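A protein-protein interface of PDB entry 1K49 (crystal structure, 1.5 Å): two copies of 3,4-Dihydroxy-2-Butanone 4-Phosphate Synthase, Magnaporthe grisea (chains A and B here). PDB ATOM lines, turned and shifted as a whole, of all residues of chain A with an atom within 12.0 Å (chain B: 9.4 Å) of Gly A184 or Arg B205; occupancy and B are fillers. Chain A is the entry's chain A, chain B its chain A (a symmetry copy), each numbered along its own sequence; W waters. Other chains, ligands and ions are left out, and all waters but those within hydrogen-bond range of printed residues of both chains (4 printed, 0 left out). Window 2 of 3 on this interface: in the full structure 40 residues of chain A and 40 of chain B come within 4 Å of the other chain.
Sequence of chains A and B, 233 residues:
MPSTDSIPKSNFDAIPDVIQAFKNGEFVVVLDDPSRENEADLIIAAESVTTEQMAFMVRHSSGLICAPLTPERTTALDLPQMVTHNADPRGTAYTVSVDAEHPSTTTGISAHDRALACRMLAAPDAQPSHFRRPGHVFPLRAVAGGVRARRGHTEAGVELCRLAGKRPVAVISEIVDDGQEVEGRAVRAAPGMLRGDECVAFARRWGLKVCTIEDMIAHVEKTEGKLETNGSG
Water W2 bridges the backbone carbonyl oxygen of Trp B206 (2.7 Å) and the backbone NH of Ala A186 (3.0 Å). Water W1 bridges NE2 of His B60 (2.8 Å) and NH1 of Arg A188 (2.9 Å). Water W3 lies within hydrogen-bond range of the backbone NH (N) of Gly A184 (2.8 Å), the backbone carbonyl oxygen (O) of Arg B205 (3.2 Å) and the side-chain carboxylate (OE1) of Glu A183 (3.2 Å). Water W4 bridges O of Arg B205 and OE2 of Glu A183.
Among the printed residues, pairs that only touch across the chains: Glu A181 with Trp B206 (3.6 Å), Val A182 with Trp B206 (3.6 Å), Gly A184 with Arg B205 (3.6 Å), Gly A184 with Trp B206 (3.6 Å), Arg A185 with Phe B56 (3.99 Å), Arg A185 with Trp B206 (3.5 Å), Ala A186 with Phe B56 (3.5 Å), Ala A186 with Leu B208 (3.99 Å), Val A187 with Phe B56 (3.6 Å) and Arg A188 with Phe B56 (3.5 Å).
Among the printed residues, 10 pairs touch across the chains. Among the printed residues, no Asp or Glu carboxylate lies within 4 Å of a Lys or Arg side-chain nitrogen of the other chain.
No position is printed for both chains.
Of chain B, only Arg B205 (3.6 Å) and Trp B206 (3.6 Å) come within 4 Å of Gly A184. Arg B205 touches just one residue of chain A: Gly A184. No residue of chain B comes within 4 Å of Glu A183. No residue of chain A comes within 4 Å of Ala B201. Trp B206 touches just these residues of chain A: Glu A181 (3.6 Å), Val A182 (3.6 Å), Gly A184 (3.6 Å) and Arg A185 (3.5 Å). No residue of chain A comes within 4 Å of Gly B207. Of the printed residues of chain B, Val A187 touches Phe B56. Of the printed residues of chain B, Arg A188 touches Phe B56 (3.5 Å). Printed residues of chain A within 4 Å of Leu B208: Ala A186. His B60 touches none of the printed residues of chain A. The nearest residue of chain A that does not touch Arg B205 is Arg A185 (5.2 Å). The nearest printed residue of chain A that does not touch Phe B56 is Val A182 (6.2 Å).
OE1 of Glu A181 sits at hydrogen-bond distance from N of Glu A183 (3.3 Å). N of Leu B208 lies within hydrogen-bond range of O of Ala B203, 3.0 Å away.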
ATOM      1  N   GLN A 180      -9.877 -29.166  -6.007  1.00  0.00           N
ATOM      2  CA  GLN A 180      -9.367 -28.852  -4.695  1.00  0.00           C
ATOM      3  C   GLN A 180      -7.990 -28.251  -4.706  1.00  0.00           C
ATOM      4  O   GLN A 180      -7.146 -28.607  -5.557  1.00  0.00           O
ATOM      5  CB  GLN A 180      -9.257 -30.159  -3.874  1.00  0.00           C
ATOM      6  CG  GLN A 180     -10.588 -30.625  -3.262  1.00  0.00           C
ATOM      7  CD  GLN A 180     -11.434 -31.378  -4.262  1.00  0.00           C
ATOM      8  OE1 GLN A 180     -12.458 -30.840  -4.719  1.00  0.00           O
ATOM      9  NE2 GLN A 180     -11.000 -32.587  -4.641  1.00  0.00           N
ATOM     10  N   GLU A 181      -7.789 -27.355  -3.749  1.00  0.00           N
ATOM     11  CA  GLU A 181      -6.491 -26.717  -3.575  1.00  0.00           C
ATOM     12  C   GLU A 181      -5.463 -27.828  -3.254  1.00  0.00           C
ATOM     13  O   GLU A 181      -5.840 -28.846  -2.702  1.00  0.00           O
ATOM     14  CB  GLU A 181      -6.533 -25.799  -2.319  1.00  0.00           C
ATOM     15  CG  GLU A 181      -5.523 -24.671  -2.405  1.00  0.00           C
ATOM     16  CD  GLU A 181      -4.586 -24.724  -1.253  1.00  0.00           C
ATOM     17  OE1 GLU A 181      -4.381 -25.802  -0.695  1.00  0.00           O
ATOM     18  OE2 GLU A 181      -4.081 -23.519  -0.946  1.00  0.00           O
ATOM     19  N   VAL A 182      -4.216 -27.612  -3.624  1.00  0.00           N
ATOM     20  CA  VAL A 182      -3.123 -28.542  -3.314  1.00  0.00           C
ATOM     21  C   VAL A 182      -2.076 -27.622  -2.732  1.00  0.00           C
ATOM     22  O   VAL A 182      -1.564 -26.775  -3.478  1.00  0.00           O
ATOM     23  CB  VAL A 182      -2.573 -29.327  -4.543  1.00  0.00           C
ATOM     24  CG1 VAL A 182      -1.398 -30.196  -4.067  1.00  0.00           C
ATOM     25  CG2 VAL A 182      -3.688 -30.185  -5.156  1.00  0.00           C
ATOM     26  N   GLU A 183      -1.824 -27.686  -1.403  1.00  0.00           N
ATOM     27  CA  GLU A 183      -0.912 -26.754  -0.798  1.00  0.00           C
ATOM     28  C   GLU A 183       0.462 -26.683  -1.487  1.00  0.00           C
ATOM     29  O   GLU A 183       1.058 -27.725  -1.756  1.00  0.00           O
ATOM     30  CB  GLU A 183      -0.767 -27.061   0.718  1.00  0.00           C
ATOM     31  CG  GLU A 183       0.361 -26.237   1.338  1.00  0.00           C
ATOM     32  CD  GLU A 183      -0.039 -24.785   1.441  1.00  0.00           C
ATOM     33  OE1 GLU A 183      -1.125 -24.319   1.109  1.00  0.00           O
ATOM     34  OE2 GLU A 183       0.957 -24.064   1.859  1.00  0.00           O
ATOM     35  N   GLY A 184       0.935 -25.470  -1.789  1.00  0.00           N
ATOM     36  CA  GLY A 184       2.237 -25.206  -2.387  1.00  0.00           C
ATOM     37  C   GLY A 184       2.513 -25.761  -3.799  1.00  0.00           C
ATOM     38  O   GLY A 184       3.676 -25.799  -4.251  1.00  0.00           O
ATOM     39  N   ARG A 185       1.450 -26.209  -4.500  1.00  0.00           N
ATOM     40  CA  ARG A 185       1.612 -26.783  -5.857  1.00  0.00           C
ATOM     41  C   ARG A 185       0.644 -26.095  -6.805  1.00  0.00           C
ATOM     42  O   ARG A 185      -0.538 -25.920  -6.475  1.00  0.00           O
ATOM     43  CB  ARG A 185       1.296 -28.275  -5.973  1.00  0.00           C
ATOM     44  CG  ARG A 185       2.062 -29.162  -4.970  1.00  0.00           C
ATOM     45  CD  ARG A 185       3.540 -29.424  -5.246  1.00  0.00           C
ATOM     46  NE  ARG A 185       4.232 -30.277  -4.255  1.00  0.00           N
ATOM     47  CZ  ARG A 185       5.560 -30.119  -4.050  1.00  0.00           C
ATOM     48  NH1 ARG A 185       6.224 -29.182  -4.728  1.00  0.00           N
ATOM     49  NH2 ARG A 185       6.221 -30.885  -3.149  1.00  0.00           N
ATOM     50  N   ALA A 186       1.165 -25.776  -7.999  1.00  0.00           N
ATOM     51  CA  ALA A 186       0.389 -25.109  -9.033  1.00  0.00           C
ATOM     52  C   ALA A 186      -0.541 -26.053  -9.795  1.00  0.00           C
ATOM     53  O   ALA A 186      -0.485 -26.150 -11.019  1.00  0.00           O
ATOM     54  CB  ALA A 186       1.256 -24.216  -9.910  1.00  0.00           C
ATOM     55  N   VAL A 187      -1.435 -26.739  -9.073  1.00  0.00           N
ATOM     56  CA  VAL A 187      -2.381 -27.611  -9.681  1.00  0.00           C
ATOM     57  C   VAL A 187      -3.632 -27.591  -8.810  1.00  0.00           C
ATOM     58  O   VAL A 187      -3.550 -27.163  -7.663  1.00  0.00           O
ATOM     59  CB  VAL A 187      -1.883 -29.068  -9.726  1.00  0.00           C
ATOM     60  CG1 VAL A 187      -0.714 -29.306 -10.687  1.00  0.00           C
ATOM     61  CG2 VAL A 187      -1.523 -29.624  -8.342  1.00  0.00           C
ATOM     62  N   ARG A 188      -4.750 -28.125  -9.319  1.00  0.00           N
ATOM     63  CA  ARG A 188      -5.994 -28.334  -8.554  1.00  0.00           C
ATOM     64  C   ARG A 188      -6.426 -29.757  -8.828  1.00  0.00           C
ATOM     65  O   ARG A 188      -6.494 -30.184  -9.991  1.00  0.00           O
ATOM     66  CB  ARG A 188      -7.197 -27.425  -8.872  1.00  0.00           C
ATOM     67  CG  ARG A 188      -6.812 -25.960  -8.953  1.00  0.00           C
ATOM     68  CD  ARG A 188      -7.045 -25.174  -7.678  1.00  0.00           C
ATOM     69  NE  ARG A 188      -8.391 -25.335  -7.138  1.00  0.00           N
ATOM     70  CZ  ARG A 188      -8.732 -24.699  -5.999  1.00  0.00           C
ATOM     71  NH1 ARG A 188      -7.856 -23.919  -5.350  1.00  0.00           N
ATOM     72  NH2 ARG A 188      -9.945 -24.869  -5.498  1.00  0.00           N
ATOM     73  N   ALA A 189      -6.767 -30.520  -7.792  1.00  0.00           N
ATOM     74  CA  ALA A 189      -7.203 -31.884  -8.012  1.00  0.00           C
ATOM     75  C   ALA A 189      -8.698 -32.003  -8.326  1.00  0.00           C
ATOM     76  O   ALA A 189      -9.529 -31.268  -7.770  1.00  0.00           O
ATOM     77  CB  ALA A 189      -6.950 -32.613  -6.691  1.00  0.00           C
ATOM     78  N   GLU B  26       6.710 -26.406 -15.927  1.00  0.00           N
ATOM     79  CA  GLU B  26       6.136 -25.632 -14.841  1.00  0.00           C
ATOM     80  C   GLU B  26       5.629 -24.292 -15.374  1.00  0.00           C
ATOM     81  O   GLU B  26       6.032 -23.793 -16.444  1.00  0.00           O
ATOM     82  CB  GLU B  26       7.171 -25.268 -13.746  1.00  0.00           C
ATOM     83  CG  GLU B  26       7.940 -26.493 -13.215  1.00  0.00           C
ATOM     84  CD  GLU B  26       8.819 -26.089 -12.058  1.00  0.00           C
ATOM     85  OE1 GLU B  26       8.609 -25.118 -11.352  1.00  0.00           O
ATOM     86  OE2 GLU B  26       9.878 -26.838 -11.924  1.00  0.00           O
ATOM     87  N   VAL B  29       6.073 -17.123 -13.608  1.00  0.00           N
ATOM     88  CA  VAL B  29       5.363 -15.840 -13.450  1.00  0.00           C
ATOM     89  C   VAL B  29       6.188 -14.775 -14.131  1.00  0.00           C
ATOM     90  O   VAL B  29       7.365 -14.542 -13.796  1.00  0.00           O
ATOM     91  CB  VAL B  29       5.114 -15.534 -11.941  1.00  0.00           C
ATOM     92  CG1 VAL B  29       4.570 -14.117 -11.740  1.00  0.00           C
ATOM     93  CG2 VAL B  29       4.204 -16.573 -11.317  1.00  0.00           C
ATOM     94  N   PHE B  56      -5.729 -24.883 -12.115  1.00  0.00           N
ATOM     95  CA  PHE B  56      -5.032 -23.936 -11.287  1.00  0.00           C
ATOM     96  C   PHE B  56      -4.946 -22.572 -12.004  1.00  0.00           C
ATOM     97  O   PHE B  56      -5.127 -21.475 -11.423  1.00  0.00           O
ATOM     98  CB  PHE B  56      -3.652 -24.483 -10.834  1.00  0.00           C
ATOM     99  CG  PHE B  56      -2.809 -23.463 -10.077  1.00  0.00           C
ATOM    100  CD1 PHE B  56      -2.835 -23.489  -8.677  1.00  0.00           C
ATOM    101  CD2 PHE B  56      -2.011 -22.482 -10.683  1.00  0.00           C
ATOM    102  CE1 PHE B  56      -2.121 -22.555  -7.920  1.00  0.00           C
ATOM    103  CE2 PHE B  56      -1.297 -21.544  -9.925  1.00  0.00           C
ATOM    104  CZ  PHE B  56      -1.321 -21.583  -8.523  1.00  0.00           C
ATOM    105  N   ARG B  59      -8.266 -20.860 -12.012  1.00  0.00           N
ATOM    106  CA  ARG B  59      -8.580 -20.349 -10.670  1.00  0.00           C
ATOM    107  C   ARG B  59      -7.807 -19.096 -10.237  1.00  0.00           C
ATOM    108  O   ARG B  59      -8.294 -18.239  -9.447  1.00  0.00           O
ATOM    109  CB  ARG B  59      -8.308 -21.434  -9.654  1.00  0.00           C
ATOM    110  CG  ARG B  59      -8.338 -20.922  -8.200  1.00  0.00           C
ATOM    111  CD  ARG B  59      -9.733 -20.523  -7.657  1.00  0.00           C
ATOM    112  NE  ARG B  59      -9.615 -20.286  -6.230  1.00  0.00           N
ATOM    113  CZ  ARG B  59      -8.970 -19.214  -5.732  1.00  0.00           C
ATOM    114  NH1 ARG B  59      -8.439 -18.264  -6.530  1.00  0.00           N
ATOM    115  NH2 ARG B  59      -8.848 -19.086  -4.385  1.00  0.00           N
ATOM    116  N   HIS B  60      -6.542 -19.023 -10.658  1.00  0.00           N
ATOM    117  CA  HIS B  60      -5.661 -17.972 -10.258  1.00  0.00           C
ATOM    118  C   HIS B  60      -5.394 -16.904 -11.336  1.00  0.00           C
ATOM    119  O   HIS B  60      -4.352 -16.228 -11.299  1.00  0.00           O
ATOM    120  CB  HIS B  60      -4.322 -18.500  -9.698  1.00  0.00           C
ATOM    121  CG  HIS B  60      -4.521 -19.267  -8.434  1.00  0.00           C
ATOM    122  ND1 HIS B  60      -4.749 -18.614  -7.225  1.00  0.00           N
ATOM    123  CD2 HIS B  60      -4.617 -20.617  -8.214  1.00  0.00           C
ATOM    124  CE1 HIS B  60      -4.922 -19.571  -6.296  1.00  0.00           C
ATOM    125  NE2 HIS B  60      -4.863 -20.789  -6.849  1.00  0.00           N
ATOM    126  N   ILE B 175      -2.614 -12.542 -14.194  1.00  0.00           N
ATOM    127  CA  ILE B 175      -2.914 -12.847 -12.814  1.00  0.00           C
ATOM    128  C   ILE B 175      -3.703 -11.693 -12.219  1.00  0.00           C
ATOM    129  O   ILE B 175      -3.134 -10.653 -11.891  1.00  0.00           O
ATOM    130  CB  ILE B 175      -1.652 -13.122 -11.989  1.00  0.00           C
ATOM    131  CG1 ILE B 175      -0.878 -14.360 -12.513  1.00  0.00           C
ATOM    132  CG2 ILE B 175      -2.073 -13.369 -10.542  1.00  0.00           C
ATOM    133  CD1 ILE B 175       0.559 -14.466 -11.989  1.00  0.00           C
ATOM    134  N   VAL B 176      -5.006 -11.919 -12.030  1.00  0.00           N
ATOM    135  CA  VAL B 176      -5.800 -10.853 -11.406  1.00  0.00           C
ATOM    136  C   VAL B 176      -5.746 -10.939  -9.877  1.00  0.00           C
ATOM    137  O   VAL B 176      -5.302 -11.935  -9.281  1.00  0.00           O
ATOM    138  CB  VAL B 176      -7.270 -10.919 -11.850  1.00  0.00           C
ATOM    139  CG1 VAL B 176      -7.317 -10.824 -13.383  1.00  0.00           C
ATOM    140  CG2 VAL B 176      -7.897 -12.220 -11.371  1.00  0.00           C
ATOM    141  N   ASP B 177      -6.212  -9.857  -9.235  1.00  0.00           N
ATOM    142  CA  ASP B 177      -6.309  -9.857  -7.780  1.00  0.00           C
ATOM    143  C   ASP B 177      -7.822 -10.016  -7.497  1.00  0.00           C
ATOM    144  O   ASP B 177      -8.586  -9.096  -7.764  1.00  0.00           O
ATOM    145  CB  ASP B 177      -5.716  -8.588  -7.133  1.00  0.00           C
ATOM    146  CG  ASP B 177      -6.000  -8.504  -5.621  1.00  0.00           C
ATOM    147  OD1 ASP B 177      -6.711  -9.271  -5.006  1.00  0.00           O
ATOM    148  OD2 ASP B 177      -5.365  -7.525  -5.057  1.00  0.00           O
ATOM    149  N   LEU B 194      -2.692  -8.239  -9.849  1.00  0.00           N
ATOM    150  CA  LEU B 194      -1.513  -8.441  -9.035  1.00  0.00           C
ATOM    151  C   LEU B 194      -0.402  -7.602  -9.585  1.00  0.00           C
ATOM    152  O   LEU B 194      -0.121  -7.680 -10.795  1.00  0.00           O
ATOM    153  CB  LEU B 194      -1.092  -9.930  -9.128  1.00  0.00           C
ATOM    154  CG  LEU B 194      -0.990 -10.656  -7.790  1.00  0.00           C
ATOM    155  CD1 LEU B 194       0.426 -10.535  -7.326  1.00  0.00           C
ATOM    156  CD2 LEU B 194      -1.932 -10.089  -6.721  1.00  0.00           C
ATOM    157  N   ASP B 197       5.537  -6.516  -6.284  1.00  0.00           N
ATOM    158  CA  ASP B 197       5.817  -7.263  -5.076  1.00  0.00           C
ATOM    159  C   ASP B 197       4.884  -8.430  -4.835  1.00  0.00           C
ATOM    160  O   ASP B 197       5.261  -9.546  -4.406  1.00  0.00           O
ATOM    161  CB  ASP B 197       5.999  -6.328  -3.854  1.00  0.00           C
ATOM    162  CG  ASP B 197       7.379  -5.685  -3.760  1.00  0.00           C
ATOM    163  OD1 ASP B 197       7.602  -4.632  -3.176  1.00  0.00           O
ATOM    164  OD2 ASP B 197       8.323  -6.373  -4.357  1.00  0.00           O
ATOM    165  N   GLU B 198       3.633  -8.126  -5.100  1.00  0.00           N
ATOM    166  CA  GLU B 198       2.661  -9.143  -4.894  1.00  0.00           C
ATOM    167  C   GLU B 198       2.984 -10.367  -5.758  1.00  0.00           C
ATOM    168  O   GLU B 198       2.760 -11.523  -5.385  1.00  0.00           O
ATOM    169  CB  GLU B 198       1.292  -8.549  -5.270  1.00  0.00           C
ATOM    170  CG  GLU B 198       0.962  -7.182  -4.636  1.00  0.00           C
ATOM    171  CD  GLU B 198      -0.518  -6.879  -4.836  1.00  0.00           C
ATOM    172  OE1 GLU B 198      -1.375  -7.234  -4.030  1.00  0.00           O
ATOM    173  OE2 GLU B 198      -0.816  -6.285  -5.982  1.00  0.00           O
ATOM    174  N   CYS B 199       3.486 -10.047  -6.957  1.00  0.00           N
ATOM    175  CA  CYS B 199       3.783 -11.066  -7.943  1.00  0.00           C
ATOM    176  C   CYS B 199       4.829 -12.066  -7.521  1.00  0.00           C
ATOM    177  O   CYS B 199       4.688 -13.286  -7.668  1.00  0.00           O
ATOM    178  CB  CYS B 199       3.932 -10.436  -9.329  1.00  0.00           C
ATOM    179  SG  CYS B 199       2.371  -9.541  -9.726  1.00  0.00           S
ATOM    180  N   VAL B 200       5.873 -11.528  -6.990  1.00  0.00           N
ATOM    181  CA  VAL B 200       6.921 -12.353  -6.481  1.00  0.00           C
ATOM    182  C   VAL B 200       6.398 -13.192  -5.320  1.00  0.00           C
ATOM    183  O   VAL B 200       6.668 -14.392  -5.267  1.00  0.00           O
ATOM    184  CB  VAL B 200       8.067 -11.475  -6.042  1.00  0.00           C
ATOM    185  CG1 VAL B 200       9.207 -12.355  -5.544  1.00  0.00           C
ATOM    186  CG2 VAL B 200       8.489 -10.639  -7.244  1.00  0.00           C
ATOM    187  N   ALA B 201       5.631 -12.557  -4.401  1.00  0.00           N
ATOM    188  CA  ALA B 201       5.077 -13.314  -3.279  1.00  0.00           C
ATOM    189  C   ALA B 201       4.179 -14.462  -3.752  1.00  0.00           C
ATOM    190  O   ALA B 201       4.197 -15.568  -3.189  1.00  0.00           O
ATOM    191  CB  ALA B 201       4.311 -12.422  -2.327  1.00  0.00           C
ATOM    192  N   PHE B 202       3.378 -14.195  -4.790  1.00  0.00           N
ATOM    193  CA  PHE B 202       2.472 -15.173  -5.394  1.00  0.00           C
ATOM    194  C   PHE B 202       3.308 -16.358  -5.942  1.00  0.00           C
ATOM    195  O   PHE B 202       3.046 -17.557  -5.719  1.00  0.00           O
ATOM    196  CB  PHE B 202       1.734 -14.480  -6.582  1.00  0.00           C
ATOM    197  CG  PHE B 202       0.905 -15.478  -7.359  1.00  0.00           C
ATOM    198  CD1 PHE B 202      -0.442 -15.715  -7.058  1.00  0.00           C
ATOM    199  CD2 PHE B 202       1.450 -16.208  -8.420  1.00  0.00           C
ATOM    200  CE1 PHE B 202      -1.258 -16.609  -7.754  1.00  0.00           C
ATOM    201  CE2 PHE B 202       0.647 -17.093  -9.152  1.00  0.00           C
ATOM    202  CZ  PHE B 202      -0.699 -17.302  -8.832  1.00  0.00           C
ATOM    203  N   ALA B 203       4.394 -15.988  -6.659  1.00  0.00           N
ATOM    204  CA  ALA B 203       5.273 -17.017  -7.193  1.00  0.00           C
ATOM    205  C   ALA B 203       5.838 -17.910  -6.066  1.00  0.00           C
ATOM    206  O   ALA B 203       5.740 -19.153  -6.115  1.00  0.00           O
ATOM    207  CB  ALA B 203       6.373 -16.393  -8.071  1.00  0.00           C
ATOM    208  N   ARG B 204       6.392 -17.287  -5.029  1.00  0.00           N
ATOM    209  CA  ARG B 204       6.961 -18.076  -3.924  1.00  0.00           C
ATOM    210  C   ARG B 204       5.964 -19.025  -3.304  1.00  0.00           C
ATOM    211  O   ARG B 204       6.272 -20.206  -3.063  1.00  0.00           O
ATOM    212  CB  ARG B 204       7.585 -17.170  -2.878  1.00  0.00           C
ATOM    213  CG  ARG B 204       8.620 -16.194  -3.477  1.00  0.00           C
ATOM    214  CD  ARG B 204       9.693 -16.923  -4.317  1.00  0.00           C
ATOM    215  NE  ARG B 204      10.713 -16.042  -4.898  1.00  0.00           N
ATOM    216  CZ  ARG B 204      11.343 -16.279  -6.053  1.00  0.00           C
ATOM    217  NH1 ARG B 204      11.085 -17.368  -6.800  1.00  0.00           N
ATOM    218  NH2 ARG B 204      12.239 -15.374  -6.434  1.00  0.00           N
ATOM    219  N   ARG B 205       4.742 -18.508  -3.045  1.00  0.00           N
ATOM    220  CA  ARG B 205       3.653 -19.291  -2.442  1.00  0.00           C
ATOM    221  C   ARG B 205       3.343 -20.610  -3.180  1.00  0.00           C
ATOM    222  O   ARG B 205       2.997 -21.656  -2.595  1.00  0.00           O
ATOM    223  CB  ARG B 205       2.380 -18.395  -2.392  1.00  0.00           C
ATOM    224  CG  ARG B 205       1.081 -19.061  -1.946  1.00  0.00           C
ATOM    225  CD  ARG B 205      -0.065 -18.040  -1.729  1.00  0.00           C
ATOM    226  NE  ARG B 205       0.463 -16.765  -1.225  1.00  0.00           N
ATOM    227  CZ  ARG B 205       0.369 -15.582  -1.853  1.00  0.00           C
ATOM    228  NH1 ARG B 205      -0.266 -15.418  -2.996  1.00  0.00           N
ATOM    229  NH2 ARG B 205       0.907 -14.495  -1.317  1.00  0.00           N
ATOM    230  N   TRP B 206       3.423 -20.519  -4.522  1.00  0.00           N
ATOM    231  CA  TRP B 206       3.129 -21.659  -5.390  1.00  0.00           C
ATOM    232  C   TRP B 206       4.362 -22.386  -5.963  1.00  0.00           C
ATOM    233  O   TRP B 206       4.207 -23.269  -6.815  1.00  0.00           O
ATOM    234  CB  TRP B 206       2.145 -21.264  -6.512  1.00  0.00           C
ATOM    235  CG  TRP B 206       0.901 -20.691  -5.922  1.00  0.00           C
ATOM    236  CD1 TRP B 206       0.486 -19.397  -5.918  1.00  0.00           C
ATOM    237  CD2 TRP B 206      -0.064 -21.459  -5.233  1.00  0.00           C
ATOM    238  NE1 TRP B 206      -0.738 -19.325  -5.288  1.00  0.00           N
ATOM    239  CE2 TRP B 206      -1.096 -20.568  -4.846  1.00  0.00           C
ATOM    240  CE3 TRP B 206      -0.141 -22.811  -4.902  1.00  0.00           C
ATOM    241  CZ2 TRP B 206      -2.184 -21.014  -4.125  1.00  0.00           C
ATOM    242  CZ3 TRP B 206      -1.261 -23.256  -4.213  1.00  0.00           C
ATOM    243  CH2 TRP B 206      -2.260 -22.366  -3.821  1.00  0.00           C
ATOM    244  N   GLY B 207       5.551 -22.036  -5.456  1.00  0.00           N
ATOM    245  CA  GLY B 207       6.781 -22.717  -5.829  1.00  0.00           C
ATOM    246  C   GLY B 207       7.145 -22.558  -7.264  1.00  0.00           C
ATOM    247  O   GLY B 207       7.669 -23.505  -7.854  1.00  0.00           O
ATOM    248  N   LEU B 208       6.881 -21.346  -7.787  1.00  0.00           N
ATOM    249  CA  LEU B 208       7.172 -21.017  -9.210  1.00  0.00           C
ATOM    250  C   LEU B 208       8.292 -20.003  -9.346  1.00  0.00           C
ATOM    251  O   LEU B 208       8.501 -19.173  -8.464  1.00  0.00           O
ATOM    252  CB  LEU B 208       5.964 -20.300  -9.844  1.00  0.00           C
ATOM    253  CG  LEU B 208       4.719 -21.121  -9.727  1.00  0.00           C
ATOM    254  CD1 LEU B 208       3.506 -20.373 -10.337  1.00  0.00           C
ATOM    255  CD2 LEU B 208       4.856 -22.535 -10.274  1.00  0.00           C
ATOM    256  N   LYS B 209       8.990 -20.035 -10.493  1.00  0.00           N
ATOM    257  CA  LYS B 209      10.008 -19.027 -10.730  1.00  0.00           C
ATOM    258  C   LYS B 209       9.272 -17.800 -11.218  1.00  0.00           C
ATOM    259  O   LYS B 209       8.136 -17.906 -11.728  1.00  0.00           O
ATOM    260  CB  LYS B 209      10.976 -19.462 -11.830  1.00  0.00           C
ATOM    261  CG  LYS B 209      11.585 -20.806 -11.476  1.00  0.00           C
ATOM    262  CD  LYS B 209      12.512 -20.659 -10.279  1.00  0.00           C
ATOM    263  CE  LYS B 209      13.004 -22.011  -9.795  1.00  0.00           C
ATOM    264  NZ  LYS B 209      13.610 -21.968  -8.461  1.00  0.00           N
ATOM    265  N   VAL B 210       9.927 -16.667 -11.040  1.00  0.00           N
ATOM    266  CA  VAL B 210       9.368 -15.358 -11.416  1.00  0.00           C
ATOM    267  C   VAL B 210      10.493 -14.490 -11.976  1.00  0.00           C
ATOM    268  O   VAL B 210      11.643 -14.517 -11.509  1.00  0.00           O
ATOM    269  CB  VAL B 210       8.712 -14.710 -10.175  1.00  0.00           C
ATOM    270  CG1 VAL B 210       9.743 -14.635  -9.041  1.00  0.00           C
ATOM    271  CG2 VAL B 210       8.168 -13.291 -10.457  1.00  0.00           C
HETATM  272  O   HOH W   1      -5.025 -23.273  -5.589  1.00  0.00           O
HETATM  273  O   HOH W   2       4.157 -25.727  -8.003  1.00  0.00           O
HETATM  274  O   HOH W   3       0.346 -22.754  -1.233  1.00  0.00           O
HETATM  275  O   HOH W   4       2.862 -22.045   0.331  1.00  0.00           O
